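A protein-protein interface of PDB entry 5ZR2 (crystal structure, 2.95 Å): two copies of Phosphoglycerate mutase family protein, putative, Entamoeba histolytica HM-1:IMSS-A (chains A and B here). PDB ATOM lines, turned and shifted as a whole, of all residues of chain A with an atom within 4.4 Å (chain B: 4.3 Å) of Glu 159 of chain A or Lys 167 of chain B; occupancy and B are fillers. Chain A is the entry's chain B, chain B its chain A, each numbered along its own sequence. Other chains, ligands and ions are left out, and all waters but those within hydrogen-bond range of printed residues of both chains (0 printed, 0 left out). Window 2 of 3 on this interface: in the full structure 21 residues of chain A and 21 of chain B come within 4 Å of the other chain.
Leu 155 of chain A touches none of the printed residues of chain B.
Glu 159 of chain A touches two residues of chain B.
Lys 167 of chain B touches just these residues of chain A: Leu 158, Glu 159, Val 186 and Leu 187.
Of the printed residues of chain A, Phe 168 of chain B touches Leu 187.
Of the printed residues of chain A, Gln 169 of chain B touches Val 186 (3.95 Å) and Leu 187 (2.8 Å).
The nearest printed residue of chain B that does not touch Glu 159 of chain A is Thr 163 of chain B (7.6 Å).
The nearest printed residue of chain A that does not touch Met 164 of chain B is Leu 155 of chain A (6.7 Å).
No position is printed for both chains.
Of the 11 pairs that touch across the chains among the printed residues, none has its exchanged pair printed and touching as well.
Glu 159 of chain A touches Met 164 of chain B.
CE of Met 164 of chain B touches CG of Met 160 of chain A, 3.5 Å away.
Val 186 of chain A touches His 166 of chain B (CG2 to O, 3.8 Å).
Val 186 of chain A touches Lys 167 of chain B.
CG1 of Val 186 of chain A touches N of Gln 169 of chain B, at 3.95 Å.
O of Leu 187 of chain A touches CA of Phe 168 of chain B, at 3.5 Å.
O of Leu 155 of chain A sits at hydrogen-bond distance from N of Met 160 of chain A (2.8 Å).
Of the 7 printed residues of chain B, 5 touch a printed residue of chain A.
Printed residues of chain B that touch a printed residue of chain A: Met 164, His 166, Lys 167, Phe 168 and Gln 169.
Hydrophobic or aromatic side chains of chain A that line the printed part of chain B: Leu 158, Met 160, Val 186 and Leu 187.
Among the printed residues, 11 pairs touch across the chains.
Among the printed residues, Asp or Glu carboxylates within 4 Å of a Lys or Arg side-chain nitrogen of the other chain: Glu 159 of chain A with Lys 167 of chain B (3.6 Å).
NZ of Lys 167 of chain B sits at hydrogen-bond distance from O of Leu 158 of chain A.
The side-chain amino group (NZ) of Lys 167 of chain B lies within salt-bridge range of the side-chain carboxylate (OE1) of Glu 159 of chain A.
The backbone carbonyl oxygen (O) of Lys 167 of chain B lies within hydrogen-bond range of the backbone NH (N) of Leu 187 of chain A (2.6 Å).
The backbone carbonyl oxygen (O) of Leu 187 of chain A sits at hydrogen-bond distance from the backbone NH (N) of Gln 169 of chain B.
The backbone carbonyl oxygen (O) of Leu 158 of chain A lies close to the side-chain sulfur (SD) of Met 164 of chain B (3.6 Å).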
ATOM      1  N   LEU A 155     -17.170 -15.686  32.670  1.00  0.00           N
ATOM      2  CA  LEU A 155     -17.126 -14.590  31.690  1.00  0.00           C
ATOM      3  C   LEU A 155     -15.779 -13.866  31.697  1.00  0.00           C
ATOM      4  O   LEU A 155     -15.203 -13.613  30.648  1.00  0.00           O
ATOM      5  CB  LEU A 155     -18.253 -13.588  31.945  1.00  0.00           C
ATOM      6  CG  LEU A 155     -19.686 -14.119  31.834  1.00  0.00           C
ATOM      7  CD1 LEU A 155     -20.684 -13.024  32.160  1.00  0.00           C
ATOM      8  CD2 LEU A 155     -19.978 -14.691  30.461  1.00  0.00           C
ATOM      9  N   GLY A 156     -15.271 -13.576  32.885  1.00  0.00           N
ATOM     10  CA  GLY A 156     -14.011 -12.856  33.043  1.00  0.00           C
ATOM     11  C   GLY A 156     -12.781 -13.631  32.601  1.00  0.00           C
ATOM     12  O   GLY A 156     -11.908 -13.081  31.928  1.00  0.00           O
ATOM     13  N   LEU A 157     -12.713 -14.904  32.991  1.00  0.00           N
ATOM     14  CA  LEU A 157     -11.635 -15.809  32.567  1.00  0.00           C
ATOM     15  C   LEU A 157     -11.652 -16.075  31.053  1.00  0.00           C
ATOM     16  O   LEU A 157     -10.606 -16.053  30.408  1.00  0.00           O
ATOM     17  CB  LEU A 157     -11.731 -17.135  33.328  1.00  0.00           C
ATOM     18  CG  LEU A 157     -11.344 -17.117  34.810  1.00  0.00           C
ATOM     19  CD1 LEU A 157     -11.857 -18.357  35.521  1.00  0.00           C
ATOM     20  CD2 LEU A 157      -9.838 -17.015  34.980  1.00  0.00           C
ATOM     21  N   LEU A 158     -12.840 -16.308  30.498  1.00  0.00           N
ATOM     22  CA  LEU A 158     -13.013 -16.559  29.055  1.00  0.00           C
ATOM     23  C   LEU A 158     -13.153 -15.287  28.204  1.00  0.00           C
ATOM     24  O   LEU A 158     -13.195 -15.371  26.972  1.00  0.00           O
ATOM     25  CB  LEU A 158     -14.228 -17.465  28.819  1.00  0.00           C
ATOM     26  CG  LEU A 158     -14.228 -18.802  29.559  1.00  0.00           C
ATOM     27  CD1 LEU A 158     -15.528 -19.552  29.326  1.00  0.00           C
ATOM     28  CD2 LEU A 158     -13.055 -19.657  29.126  1.00  0.00           C
ATOM     29  N   GLU A 159     -13.255 -14.134  28.869  1.00  0.00           N
ATOM     30  CA  GLU A 159     -13.287 -12.809  28.229  1.00  0.00           C
ATOM     31  C   GLU A 159     -14.526 -12.654  27.350  1.00  0.00           C
ATOM     32  O   GLU A 159     -14.432 -12.388  26.153  1.00  0.00           O
ATOM     33  CB  GLU A 159     -11.991 -12.519  27.458  1.00  0.00           C
ATOM     34  CG  GLU A 159     -10.766 -12.465  28.354  1.00  0.00           C
ATOM     35  CD  GLU A 159      -9.479 -12.244  27.584  1.00  0.00           C
ATOM     36  OE1 GLU A 159      -9.170 -13.059  26.688  1.00  0.00           O
ATOM     37  OE2 GLU A 159      -8.765 -11.264  27.885  1.00  0.00           O
ATOM     38  N   MET A 160     -15.682 -12.820  27.984  1.00  0.00           N
ATOM     39  CA  MET A 160     -16.980 -12.798  27.319  1.00  0.00           C
ATOM     40  C   MET A 160     -17.760 -11.544  27.678  1.00  0.00           C
ATOM     41  O   MET A 160     -17.528 -10.929  28.718  1.00  0.00           O
ATOM     42  CB  MET A 160     -17.797 -14.021  27.730  1.00  0.00           C
ATOM     43  CG  MET A 160     -17.387 -15.312  27.044  1.00  0.00           C
ATOM     44  SD  MET A 160     -18.121 -16.748  27.859  1.00  0.00           S
ATOM     45  CE  MET A 160     -17.461 -18.088  26.874  1.00  0.00           C
ATOM     46  N   PRO A 185      -7.013 -19.314  29.991  1.00  0.00           N
ATOM     47  CA  PRO A 185      -7.854 -20.349  30.580  1.00  0.00           C
ATOM     48  C   PRO A 185      -8.781 -21.018  29.572  1.00  0.00           C
ATOM     49  O   PRO A 185      -9.345 -20.349  28.706  1.00  0.00           O
ATOM     50  CB  PRO A 185      -8.685 -19.583  31.629  1.00  0.00           C
ATOM     51  CG  PRO A 185      -8.310 -18.143  31.493  1.00  0.00           C
ATOM     52  CD  PRO A 185      -7.627 -17.990  30.173  1.00  0.00           C
ATOM     53  N   VAL A 186      -8.943 -22.328  29.721  1.00  0.00           N
ATOM     54  CA  VAL A 186      -9.806 -23.131  28.852  1.00  0.00           C
ATOM     55  C   VAL A 186     -10.819 -23.873  29.726  1.00  0.00           C
ATOM     56  O   VAL A 186     -10.429 -24.593  30.650  1.00  0.00           O
ATOM     57  CB  VAL A 186      -8.984 -24.144  28.028  1.00  0.00           C
ATOM     58  CG1 VAL A 186      -9.870 -24.912  27.060  1.00  0.00           C
ATOM     59  CG2 VAL A 186      -7.880 -23.440  27.253  1.00  0.00           C
ATOM     60  N   LEU A 187     -12.105 -23.687  29.421  1.00  0.00           N
ATOM     61  CA  LEU A 187     -13.203 -24.363  30.113  1.00  0.00           C
ATOM     62  C   LEU A 187     -13.231 -25.852  29.750  1.00  0.00           C
ATOM     63  O   LEU A 187     -13.363 -26.201  28.579  1.00  0.00           O
ATOM     64  CB  LEU A 187     -14.543 -23.710  29.741  1.00  0.00           C
ATOM     65  CG  LEU A 187     -15.820 -24.176  30.463  1.00  0.00           C
ATOM     66  CD1 LEU A 187     -15.846 -23.685  31.898  1.00  0.00           C
ATOM     67  CD2 LEU A 187     -17.067 -23.698  29.733  1.00  0.00           C
ATOM     68  N   THR B 163     -13.416 -17.308  17.992  1.00  0.00           N
ATOM     69  CA  THR B 163     -12.208 -17.557  18.792  1.00  0.00           C
ATOM     70  C   THR B 163     -12.482 -18.153  20.187  1.00  0.00           C
ATOM     71  O   THR B 163     -11.558 -18.640  20.844  1.00  0.00           O
ATOM     72  CB  THR B 163     -11.366 -16.273  18.943  1.00  0.00           C
ATOM     73  OG1 THR B 163     -12.169 -15.234  19.517  1.00  0.00           O
ATOM     74  CG2 THR B 163     -10.833 -15.822  17.586  1.00  0.00           C
ATOM     75  N   MET B 164     -13.737 -18.097  20.637  1.00  0.00           N
ATOM     76  CA  MET B 164     -14.176 -18.806  21.846  1.00  0.00           C
ATOM     77  C   MET B 164     -14.081 -20.329  21.705  1.00  0.00           C
ATOM     78  O   MET B 164     -13.975 -21.025  22.713  1.00  0.00           O
ATOM     79  CB  MET B 164     -15.618 -18.434  22.210  1.00  0.00           C
ATOM     80  CG  MET B 164     -15.852 -16.975  22.558  1.00  0.00           C
ATOM     81  SD  MET B 164     -15.008 -16.442  24.054  1.00  0.00           S
ATOM     82  CE  MET B 164     -15.533 -14.741  24.093  1.00  0.00           C
ATOM     83  N   TYR B 165     -14.125 -20.835  20.471  1.00  0.00           N
ATOM     84  CA  TYR B 165     -13.877 -22.253  20.166  1.00  0.00           C
ATOM     85  C   TYR B 165     -12.667 -22.827  20.911  1.00  0.00           C
ATOM     86  O   TYR B 165     -12.731 -23.933  21.430  1.00  0.00           O
ATOM     87  CB  TYR B 165     -13.689 -22.417  18.652  1.00  0.00           C
ATOM     88  CG  TYR B 165     -13.461 -23.827  18.116  1.00  0.00           C
ATOM     89  CD1 TYR B 165     -12.187 -24.388  18.110  1.00  0.00           C
ATOM     90  CD2 TYR B 165     -14.505 -24.564  17.545  1.00  0.00           C
ATOM     91  CE1 TYR B 165     -11.958 -25.651  17.600  1.00  0.00           C
ATOM     92  CE2 TYR B 165     -14.283 -25.832  17.025  1.00  0.00           C
ATOM     93  CZ  TYR B 165     -13.004 -26.373  17.058  1.00  0.00           C
ATOM     94  OH  TYR B 165     -12.744 -27.635  16.557  1.00  0.00           O
ATOM     95  N   HIS B 166     -11.581 -22.066  20.990  1.00  0.00           N
ATOM     96  CA  HIS B 166     -10.331 -22.560  21.598  1.00  0.00           C
ATOM     97  C   HIS B 166     -10.306 -22.529  23.134  1.00  0.00           C
ATOM     98  O   HIS B 166      -9.339 -22.984  23.745  1.00  0.00           O
ATOM     99  CB  HIS B 166      -9.133 -21.790  21.038  1.00  0.00           C
ATOM    100  CG  HIS B 166      -9.139 -21.684  19.546  1.00  0.00           C
ATOM    101  ND1 HIS B 166      -9.043 -22.785  18.722  1.00  0.00           N
ATOM    102  CD2 HIS B 166      -9.268 -20.612  18.731  1.00  0.00           C
ATOM    103  CE1 HIS B 166      -9.097 -22.393  17.461  1.00  0.00           C
ATOM    104  NE2 HIS B 166      -9.234 -21.079  17.440  1.00  0.00           N
ATOM    105  N   LYS B 167     -11.366 -21.990  23.736  1.00  0.00           N
ATOM    106  CA  LYS B 167     -11.530 -21.904  25.188  1.00  0.00           C
ATOM    107  C   LYS B 167     -12.492 -22.952  25.771  1.00  0.00           C
ATOM    108  O   LYS B 167     -12.702 -22.981  26.984  1.00  0.00           O
ATOM    109  CB  LYS B 167     -12.030 -20.510  25.548  1.00  0.00           C
ATOM    110  CG  LYS B 167     -11.091 -19.391  25.144  1.00  0.00           C
ATOM    111  CD  LYS B 167     -11.763 -18.037  25.266  1.00  0.00           C
ATOM    112  CE  LYS B 167     -10.920 -16.947  24.628  1.00  0.00           C
ATOM    113  NZ  LYS B 167     -11.176 -15.621  25.251  1.00  0.00           N
ATOM    114  N   PHE B 168     -13.070 -23.791  24.911  1.00  0.00           N
ATOM    115  CA  PHE B 168     -13.870 -24.948  25.327  1.00  0.00           C
ATOM    116  C   PHE B 168     -13.110 -26.207  24.975  1.00  0.00           C
ATOM    117  O   PHE B 168     -12.673 -26.354  23.843  1.00  0.00           O
ATOM    118  CB  PHE B 168     -15.203 -24.989  24.583  1.00  0.00           C
ATOM    119  CG  PHE B 168     -16.182 -23.933  25.010  1.00  0.00           C
ATOM    120  CD1 PHE B 168     -16.073 -22.640  24.527  1.00  0.00           C
ATOM    121  CD2 PHE B 168     -17.232 -24.235  25.872  1.00  0.00           C
ATOM    122  CE1 PHE B 168     -16.978 -21.660  24.903  1.00  0.00           C
ATOM    123  CE2 PHE B 168     -18.141 -23.261  26.254  1.00  0.00           C
ATOM    124  CZ  PHE B 168     -18.016 -21.973  25.766  1.00  0.00           C
ATOM    125  N   GLN B 169     -12.957 -27.113  25.937  1.00  0.00           N
ATOM    126  CA  GLN B 169     -12.409 -28.444  25.667  1.00  0.00           C
ATOM    127  C   GLN B 169     -13.462 -29.488  25.995  1.00  0.00           C
ATOM    128  O   GLN B 169     -14.021 -29.488  27.089  1.00  0.00           O
ATOM    129  CB  GLN B 169     -11.147 -28.698  26.476  1.00  0.00           C
ATOM    130  CG  GLN B 169     -10.394 -29.944  26.040  1.00  0.00           C
ATOM    131  CD  GLN B 169      -9.077 -30.100  26.768  1.00  0.00           C
ATOM    132  OE1 GLN B 169      -8.009 -30.004  26.167  1.00  0.00           O
ATOM    133  NE2 GLN B 169      -9.144 -30.333  28.076  1.00  0.00           N
